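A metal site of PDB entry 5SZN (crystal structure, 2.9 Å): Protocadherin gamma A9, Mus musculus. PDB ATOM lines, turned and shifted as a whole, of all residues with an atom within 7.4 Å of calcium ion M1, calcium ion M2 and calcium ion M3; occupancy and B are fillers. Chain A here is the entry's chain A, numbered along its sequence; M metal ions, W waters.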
ATOM      1  N   GLU A 116      -4.200  -3.256 -22.087  1.00  0.00           N
ATOM      2  CA  GLU A 116      -5.095  -2.102 -22.041  1.00  0.00           C
ATOM      3  C   GLU A 116      -4.706  -1.063 -23.094  1.00  0.00           C
ATOM      4  O   GLU A 116      -5.567  -0.320 -23.576  1.00  0.00           O
ATOM      5  CB  GLU A 116      -5.069  -1.491 -20.641  1.00  0.00           C
ATOM      6  CG  GLU A 116      -6.070  -0.377 -20.405  1.00  0.00           C
ATOM      7  CD  GLU A 116      -5.951   0.196 -19.001  1.00  0.00           C
ATOM      8  OE1 GLU A 116      -5.221  -0.397 -18.178  1.00  0.00           O
ATOM      9  OE2 GLU A 116      -6.582   1.243 -18.735  1.00  0.00           O
ATOM     10  N   LEU A 172      -9.827  -1.529 -25.035  1.00  0.00           N
ATOM     11  CA  LEU A 172     -10.215  -2.152 -23.777  1.00  0.00           C
ATOM     12  C   LEU A 172      -9.769  -1.295 -22.593  1.00  0.00           C
ATOM     13  O   LEU A 172      -8.891  -0.438 -22.699  1.00  0.00           O
ATOM     14  CB  LEU A 172      -9.621  -3.547 -23.652  1.00  0.00           C
ATOM     15  CG  LEU A 172     -10.219  -4.594 -24.610  1.00  0.00           C
ATOM     16  CD1 LEU A 172      -9.686  -5.975 -24.285  1.00  0.00           C
ATOM     17  CD2 LEU A 172     -11.742  -4.572 -24.529  1.00  0.00           C
ATOM     18  N   ASP A 173     -10.417  -1.532 -21.453  1.00  0.00           N
ATOM     19  CA  ASP A 173     -10.069  -0.839 -20.207  1.00  0.00           C
ATOM     20  C   ASP A 173     -10.293  -1.799 -19.058  1.00  0.00           C
ATOM     21  O   ASP A 173     -11.420  -2.241 -18.817  1.00  0.00           O
ATOM     22  CB  ASP A 173     -10.915   0.427 -20.020  1.00  0.00           C
ATOM     23  CG  ASP A 173     -10.442   1.272 -18.868  1.00  0.00           C
ATOM     24  OD1 ASP A 173      -9.216   1.471 -18.728  1.00  0.00           O
ATOM     25  OD2 ASP A 173     -11.295   1.743 -18.082  1.00  0.00           O
ATOM     26  N   ARG A 174      -9.212  -2.137 -18.341  1.00  0.00           N
ATOM     27  CA  ARG A 174      -9.315  -3.079 -17.242  1.00  0.00           C
ATOM     28  C   ARG A 174      -9.957  -2.450 -16.001  1.00  0.00           C
ATOM     29  O   ARG A 174     -10.480  -3.183 -15.163  1.00  0.00           O
ATOM     30  CB  ARG A 174      -7.936  -3.613 -16.875  1.00  0.00           C
ATOM     31  CG  ARG A 174      -7.005  -2.556 -16.340  1.00  0.00           C
ATOM     32  CD  ARG A 174      -5.809  -3.162 -15.634  1.00  0.00           C
ATOM     33  NE  ARG A 174      -6.195  -3.967 -14.481  1.00  0.00           N
ATOM     34  CZ  ARG A 174      -6.356  -3.489 -13.252  1.00  0.00           C
ATOM     35  NH1 ARG A 174      -6.186  -2.197 -13.016  1.00  0.00           N
ATOM     36  NH2 ARG A 174      -6.706  -4.297 -12.266  1.00  0.00           N
ATOM     37  N   GLU A 175      -9.920  -1.120 -15.887  1.00  0.00           N
ATOM     38  CA  GLU A 175     -10.441  -0.473 -14.695  1.00  0.00           C
ATOM     39  C   GLU A 175     -11.962  -0.592 -14.612  1.00  0.00           C
ATOM     40  O   GLU A 175     -12.527  -0.586 -13.517  1.00  0.00           O
ATOM     41  CB  GLU A 175     -10.031   0.998 -14.667  1.00  0.00           C
ATOM     42  CG  GLU A 175      -8.597   1.218 -14.216  1.00  0.00           C
ATOM     43  CD  GLU A 175      -7.580   0.612 -15.152  1.00  0.00           C
ATOM     44  OE1 GLU A 175      -7.776   0.700 -16.385  1.00  0.00           O
ATOM     45  OE2 GLU A 175      -6.586   0.027 -14.674  1.00  0.00           O
ATOM     46  N   GLU A 176     -12.630  -0.716 -15.757  1.00  0.00           N
ATOM     47  CA  GLU A 176     -14.074  -0.900 -15.777  1.00  0.00           C
ATOM     48  C   GLU A 176     -14.455  -2.370 -15.708  1.00  0.00           C
ATOM     49  O   GLU A 176     -15.393  -2.744 -14.990  1.00  0.00           O
ATOM     50  CB  GLU A 176     -14.666  -0.268 -17.039  1.00  0.00           C
ATOM     51  CG  GLU A 176     -14.171   1.145 -17.317  1.00  0.00           C
ATOM     52  CD  GLU A 176     -14.684   1.706 -18.631  1.00  0.00           C
ATOM     53  OE1 GLU A 176     -15.691   1.178 -19.148  1.00  0.00           O
ATOM     54  OE2 GLU A 176     -14.075   2.663 -19.139  1.00  0.00           O
ATOM     55  N   LEU A 205      -4.681  -6.913 -19.740  1.00  0.00           N
ATOM     56  CA  LEU A 205      -3.470  -6.592 -18.996  1.00  0.00           C
ATOM     57  C   LEU A 205      -3.597  -5.193 -18.387  1.00  0.00           C
ATOM     58  O   LEU A 205      -4.607  -4.498 -18.550  1.00  0.00           O
ATOM     59  CB  LEU A 205      -2.236  -6.700 -19.892  1.00  0.00           C
ATOM     60  CG  LEU A 205      -1.928  -8.091 -20.441  1.00  0.00           C
ATOM     61  CD1 LEU A 205      -0.581  -8.093 -21.161  1.00  0.00           C
ATOM     62  CD2 LEU A 205      -1.959  -9.139 -19.341  1.00  0.00           C
ATOM     63  N   ASP A 206      -2.559  -4.767 -17.678  1.00  0.00           N
ATOM     64  CA  ASP A 206      -2.583  -3.516 -16.945  1.00  0.00           C
ATOM     65  C   ASP A 206      -1.553  -2.551 -17.530  1.00  0.00           C
ATOM     66  O   ASP A 206      -0.368  -2.881 -17.626  1.00  0.00           O
ATOM     67  CB  ASP A 206      -2.309  -3.731 -15.454  1.00  0.00           C
ATOM     68  CG  ASP A 206      -2.500  -2.463 -14.635  1.00  0.00           C
ATOM     69  OD1 ASP A 206      -3.145  -1.525 -15.142  1.00  0.00           O
ATOM     70  OD2 ASP A 206      -2.021  -2.421 -13.482  1.00  0.00           O
ATOM     71  N   THR A 207      -2.020  -1.372 -17.920  1.00  0.00           N
ATOM     72  CA  THR A 207      -1.160  -0.265 -18.314  1.00  0.00           C
ATOM     73  C   THR A 207      -1.252   0.819 -17.250  1.00  0.00           C
ATOM     74  O   THR A 207      -2.341   1.116 -16.744  1.00  0.00           O
ATOM     75  CB  THR A 207      -1.572   0.305 -19.683  1.00  0.00           C
ATOM     76  OG1 THR A 207      -1.465  -0.715 -20.683  1.00  0.00           O
ATOM     77  CG2 THR A 207      -0.675   1.482 -20.062  1.00  0.00           C
ATOM     78  N   ASN A 208      -0.112   1.402 -16.898  1.00  0.00           N
ATOM     79  CA  ASN A 208      -0.071   2.474 -15.909  1.00  0.00           C
ATOM     80  C   ASN A 208      -0.603   3.754 -16.565  1.00  0.00           C
ATOM     81  O   ASN A 208       0.144   4.651 -16.950  1.00  0.00           O
ATOM     82  CB  ASN A 208       1.347   2.655 -15.372  1.00  0.00           C
ATOM     83  CG  ASN A 208       1.397   3.555 -14.157  1.00  0.00           C
ATOM     84  OD1 ASN A 208       0.367   3.884 -13.569  1.00  0.00           O
ATOM     85  ND2 ASN A 208       2.606   3.943 -13.757  1.00  0.00           N
ATOM     86  N   ASP A 209      -1.921   3.809 -16.688  1.00  0.00           N
ATOM     87  CA  ASP A 209      -2.606   4.978 -17.242  1.00  0.00           C
ATOM     88  C   ASP A 209      -3.479   5.674 -16.201  1.00  0.00           C
ATOM     89  O   ASP A 209      -4.238   6.593 -16.548  1.00  0.00           O
ATOM     90  CB  ASP A 209      -3.438   4.581 -18.463  1.00  0.00           C
ATOM     91  CG  ASP A 209      -4.474   3.526 -18.152  1.00  0.00           C
ATOM     92  OD1 ASP A 209      -4.396   2.905 -17.084  1.00  0.00           O
ATOM     93  OD2 ASP A 209      -5.368   3.312 -18.998  1.00  0.00           O
ATOM     94  N   ASN A 210      -3.404   5.258 -14.933  1.00  0.00           N
ATOM     95  CA  ASN A 210      -4.133   5.877 -13.844  1.00  0.00           C
ATOM     96  C   ASN A 210      -3.145   6.588 -12.926  1.00  0.00           C
ATOM     97  O   ASN A 210      -2.297   5.950 -12.303  1.00  0.00           O
ATOM     98  CB  ASN A 210      -4.935   4.840 -13.050  1.00  0.00           C
ATOM     99  CG  ASN A 210      -6.086   4.272 -13.839  1.00  0.00           C
ATOM    100  OD1 ASN A 210      -5.971   3.211 -14.461  1.00  0.00           O
ATOM    101  ND2 ASN A 210      -7.218   4.970 -13.818  1.00  0.00           N
ATOM    102  N   ALA A 211      -3.271   7.925 -12.850  1.00  0.00           N
ATOM    103  CA  ALA A 211      -2.450   8.681 -11.923  1.00  0.00           C
ATOM    104  C   ALA A 211      -3.116   8.762 -10.559  1.00  0.00           C
ATOM    105  O   ALA A 211      -4.351   8.730 -10.462  1.00  0.00           O
ATOM    106  CB  ALA A 211      -2.206  10.092 -12.458  1.00  0.00           C
ATOM    107  N   PRO A 212      -2.340   8.847  -9.481  1.00  0.00           N
ATOM    108  CA  PRO A 212      -2.950   8.967  -8.152  1.00  0.00           C
ATOM    109  C   PRO A 212      -3.744  10.257  -8.026  1.00  0.00           C
ATOM    110  O   PRO A 212      -3.296  11.327  -8.449  1.00  0.00           O
ATOM    111  CB  PRO A 212      -1.740   8.959  -7.210  1.00  0.00           C
ATOM    112  CG  PRO A 212      -0.640   8.312  -7.990  1.00  0.00           C
ATOM    113  CD  PRO A 212      -0.877   8.719  -9.413  1.00  0.00           C
ATOM    114  N   SER A 239      -5.993   7.679  -4.628  1.00  0.00           N
ATOM    115  CA  SER A 239      -6.665   6.627  -5.380  1.00  0.00           C
ATOM    116  C   SER A 239      -5.821   6.248  -6.592  1.00  0.00           C
ATOM    117  O   SER A 239      -5.490   7.104  -7.411  1.00  0.00           O
ATOM    118  CB  SER A 239      -8.063   7.059  -5.812  1.00  0.00           C
ATOM    119  OG  SER A 239      -8.879   7.359  -4.702  1.00  0.00           O
ATOM    120  N   ASP A 240      -5.470   4.967  -6.683  1.00  0.00           N
ATOM    121  CA  ASP A 240      -4.781   4.432  -7.862  1.00  0.00           C
ATOM    122  C   ASP A 240      -5.397   3.077  -8.191  1.00  0.00           C
ATOM    123  O   ASP A 240      -5.006   2.045  -7.603  1.00  0.00           O
ATOM    124  CB  ASP A 240      -3.280   4.306  -7.624  1.00  0.00           C
ATOM    125  CG  ASP A 240      -2.486   4.287  -8.924  1.00  0.00           C
ATOM    126  OD1 ASP A 240      -3.086   4.011  -9.981  1.00  0.00           O
ATOM    127  OD2 ASP A 240      -1.267   4.552  -8.878  1.00  0.00           O
ATOM    128  N   PRO A 241      -6.359   3.033  -9.113  1.00  0.00           N
ATOM    129  CA  PRO A 241      -7.019   1.761  -9.441  1.00  0.00           C
ATOM    130  C   PRO A 241      -6.145   0.781 -10.212  1.00  0.00           C
ATOM    131  O   PRO A 241      -6.623  -0.314 -10.530  1.00  0.00           O
ATOM    132  CB  PRO A 241      -8.220   2.199 -10.298  1.00  0.00           C
ATOM    133  CG  PRO A 241      -8.367   3.669 -10.042  1.00  0.00           C
ATOM    134  CD  PRO A 241      -6.982   4.174  -9.795  1.00  0.00           C
ATOM    135  N   ASP A 242      -4.890   1.119 -10.511  1.00  0.00           N
ATOM    136  CA  ASP A 242      -4.016   0.214 -11.234  1.00  0.00           C
ATOM    137  C   ASP A 242      -3.696  -1.014 -10.389  1.00  0.00           C
ATOM    138  O   ASP A 242      -4.175  -1.178  -9.261  1.00  0.00           O
ATOM    139  CB  ASP A 242      -2.731   0.937 -11.651  1.00  0.00           C
ATOM    140  CG  ASP A 242      -2.957   1.917 -12.775  1.00  0.00           C
ATOM    141  OD1 ASP A 242      -3.735   1.600 -13.698  1.00  0.00           O
ATOM    142  OD2 ASP A 242      -2.356   3.012 -12.744  1.00  0.00           O
ATOM    143  N   GLU A 243      -2.866  -1.886 -10.943  1.00  0.00           N
ATOM    144  CA  GLU A 243      -2.532  -3.166 -10.324  1.00  0.00           C
ATOM    145  C   GLU A 243      -1.031  -3.270 -10.111  1.00  0.00           C
ATOM    146  O   GLU A 243      -0.241  -2.898 -10.986  1.00  0.00           O
ATOM    147  CB  GLU A 243      -3.029  -4.336 -11.195  1.00  0.00           C
ATOM    148  CG  GLU A 243      -2.840  -5.704 -10.560  1.00  0.00           C
ATOM    149  CD  GLU A 243      -3.493  -6.793 -11.378  1.00  0.00           C
ATOM    150  OE1 GLU A 243      -4.128  -6.478 -12.405  1.00  0.00           O
ATOM    151  OE2 GLU A 243      -3.386  -7.980 -10.993  1.00  0.00           O
ATOM    152  N   ALA A 245       2.694  -2.488  -8.570  1.00  0.00           N
ATOM    153  CA  ALA A 245       3.421  -1.276  -8.214  1.00  0.00           C
ATOM    154  C   ALA A 245       2.775  -0.038  -8.807  1.00  0.00           C
ATOM    155  O   ALA A 245       2.926   1.063  -8.267  1.00  0.00           O
ATOM    156  CB  ALA A 245       4.877  -1.384  -8.658  1.00  0.00           C
ATOM    157  N   ASN A 246       2.023  -0.201  -9.894  1.00  0.00           N
ATOM    158  CA  ASN A 246       1.310   0.921 -10.482  1.00  0.00           C
ATOM    159  C   ASN A 246       0.123   1.352  -9.641  1.00  0.00           C
ATOM    160  O   ASN A 246      -0.473   2.388  -9.935  1.00  0.00           O
ATOM    161  CB  ASN A 246       0.834   0.565 -11.891  1.00  0.00           C
ATOM    162  CG  ASN A 246       1.979   0.163 -12.804  1.00  0.00           C
ATOM    163  OD1 ASN A 246       3.121   0.596 -12.616  1.00  0.00           O
ATOM    164  ND2 ASN A 246       1.676  -0.644 -13.804  1.00  0.00           N
ATOM    165  N   GLY A 247      -0.245   0.588  -8.610  1.00  0.00           N
ATOM    166  CA  GLY A 247      -1.344   0.968  -7.737  1.00  0.00           C
ATOM    167  C   GLY A 247      -0.871   1.341  -6.346  1.00  0.00           C
ATOM    168  O   GLY A 247      -1.680   1.688  -5.481  1.00  0.00           O
ATOM    169  N   LYS A 248       0.438   1.268  -6.120  1.00  0.00           N
ATOM    170  CA  LYS A 248       1.030   1.633  -4.836  1.00  0.00           C
ATOM    171  C   LYS A 248       1.213   3.136  -4.749  1.00  0.00           C
ATOM    172  O   LYS A 248       1.366   3.824  -5.757  1.00  0.00           O
ATOM    173  CB  LYS A 248       2.370   0.913  -4.654  1.00  0.00           C
ATOM    174  CG  LYS A 248       3.009   1.099  -3.298  1.00  0.00           C
ATOM    175  CD  LYS A 248       2.102   0.616  -2.179  1.00  0.00           C
ATOM    176  CE  LYS A 248       2.610   1.065  -0.824  1.00  0.00           C
ATOM    177  NZ  LYS A 248       4.025   0.624  -0.601  1.00  0.00           N
ATOM    178  N   GLU A 294       3.065   9.376  -5.423  1.00  0.00           N
ATOM    179  CA  GLU A 294       3.550   8.745  -6.639  1.00  0.00           C
ATOM    180  C   GLU A 294       3.300   7.251  -6.587  1.00  0.00           C
ATOM    181  O   GLU A 294       3.153   6.660  -5.513  1.00  0.00           O
ATOM    182  CB  GLU A 294       5.042   9.019  -6.866  1.00  0.00           C
ATOM    183  CG  GLU A 294       5.369  10.464  -7.197  1.00  0.00           C
ATOM    184  CD  GLU A 294       6.851  10.707  -7.383  1.00  0.00           C
ATOM    185  OE1 GLU A 294       7.576   9.740  -7.715  1.00  0.00           O
ATOM    186  OE2 GLU A 294       7.298  11.857  -7.194  1.00  0.00           O
ATOM    187  N   ASP A 295       3.260   6.633  -7.761  1.00  0.00           N
ATOM    188  CA  ASP A 295       3.024   5.211  -7.920  1.00  0.00           C
ATOM    189  C   ASP A 295       4.325   4.519  -8.343  1.00  0.00           C
ATOM    190  O   ASP A 295       5.421   5.010  -8.024  1.00  0.00           O
ATOM    191  CB  ASP A 295       1.866   5.009  -8.889  1.00  0.00           C
ATOM    192  CG  ASP A 295       2.127   5.631 -10.248  1.00  0.00           C
ATOM    193  OD1 ASP A 295       3.140   6.346 -10.394  1.00  0.00           O
ATOM    194  OD2 ASP A 295       1.302   5.420 -11.171  1.00  0.00           O
ATOM    195  N   GLY A 296       4.210   3.387  -9.042  1.00  0.00           N
ATOM    196  CA  GLY A 296       5.403   2.714  -9.530  1.00  0.00           C
ATOM    197  C   GLY A 296       6.132   3.520 -10.585  1.00  0.00           C
ATOM    198  O   GLY A 296       7.371   3.586 -10.578  1.00  0.00           O
ATOM    199  N   GLY A 297       5.394   4.132 -11.506  1.00  0.00           N
ATOM    200  CA  GLY A 297       5.971   4.997 -12.507  1.00  0.00           C
ATOM    201  C   GLY A 297       6.059   6.442 -12.033  1.00  0.00           C
ATOM    202  O   GLY A 297       5.894   6.749 -10.851  1.00  0.00           O
ATOM    203  N   LEU A 299       4.049   8.702 -12.452  1.00  0.00           N
ATOM    204  CA  LEU A 299       2.731   9.299 -12.302  1.00  0.00           C
ATOM    205  C   LEU A 299       2.566   9.833 -10.878  1.00  0.00           C
ATOM    206  O   LEU A 299       2.868   9.130  -9.902  1.00  0.00           O
ATOM    207  CB  LEU A 299       1.641   8.276 -12.630  1.00  0.00           C
ATOM    208  CG  LEU A 299       1.364   7.955 -14.098  1.00  0.00           C
ATOM    209  CD1 LEU A 299       2.491   7.145 -14.714  1.00  0.00           C
ATOM    210  CD2 LEU A 299       0.045   7.213 -14.247  1.00  0.00           C
HETATM  211 CA    CA M   1      -0.919   4.159 -11.502  1.00  0.00          CA
HETATM  212 CA    CA M   2      -4.868   0.527 -15.926  1.00  0.00          CA
HETATM  213 CA    CA M   3      -7.537   2.810 -17.629  1.00  0.00          CA
HETATM  214  O   HOH W   1      -7.642   5.823 -19.077  1.00  0.00           O
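Calcium ion M3 is bound by OE2 of Glu 116, OD1 of Asp 173, OE1 of Glu 175 and OD2 of Asp 209. Calcium ion M3 has four donor atoms within binding distance.
The nearest printed residue that does not touch calcium ion M1 is Leu 299 (4.2 Å).
OD1 of Asn 210 sits close to OE2 of Glu 175 (3.2 Å). OD1 of Asn 210 sits close to OD1 of Asp 209, 3.1 Å away. OD1 of Asp 295 sits at hydrogen-bond distance from N of Leu 299, 3.3 Å away. The side-chain carboxylate (OD1) of Asp 295 sits close to the backbone NH (N) of Gly 297 (3.3 Å). OD1 of Asp 206 sits close to NH1 of Arg 174 (3.8 Å). The backbone NH (N) of Glu 243 sits at hydrogen-bond distance from the side-chain carboxylate (OD2) of Asp 206, at 2.7 Å. The guanidinium group (NH1) of Arg 174 sits at hydrogen-bond distance from the backbone carbonyl oxygen (O) of Pro 241, 3.1 Å away. The side-chain carboxylate (OE1) of Glu 243 lies within salt-bridge range of the guanidinium group (NH2) of Arg 174 (3.4 Å).
Calcium ion M1 is bound by the side-chain carboxylate (OD2) of Asp 242, the backbone carbonyl oxygen (O) of Asn 210, the backbone carbonyl oxygen (O) of Asn 246, the side-chain amide oxygen (OD1) of Asn 208, the side-chain carboxylate (OD2) of Asp 295, the side-chain carboxylate (OD1) of Asp 240 and the side-chain carboxylate (OD2) of Asp 240.
Merely in contact with calcium ion M2: Arg 174 (3.8 Å). Within 4 Å of calcium ion M2: Glu 116, Arg 174, Glu 175, Asp 206, Thr 207, Asp 209, Asn 210 and Asp 242. The nearest printed residue that does not touch calcium ion M2 is Asn 208 (4.9 Å).
Of the 28 residues printed, 5 come within 4 Å of calcium ion M3. The nearest printed residue that does not touch calcium ion M3 is Arg 174 (5.3 Å).
Calcium ion M2 is bound by OE2 of Glu 175 (2.2 Å). The side-chain carboxylate (OE1) of Glu 116 binds calcium ion M2 (2.5 Å). The side-chain carboxylate (OD1) of Asp 209 is bound to calcium ion M2, 2.7 Å away. Calcium ion M2 is bound by the side-chain carboxylate (OD1) of Asp 242 (2.7 Å). Calcium ion M2 is bound by the backbone carbonyl oxygen (O) of Thr 207, at 2.7 Å. Calcium ion M2 is bound by OD1 of Asp 206. The side-chain carboxylate (OE1) of Glu 175 binds calcium ion M2, at 2.9 Å.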
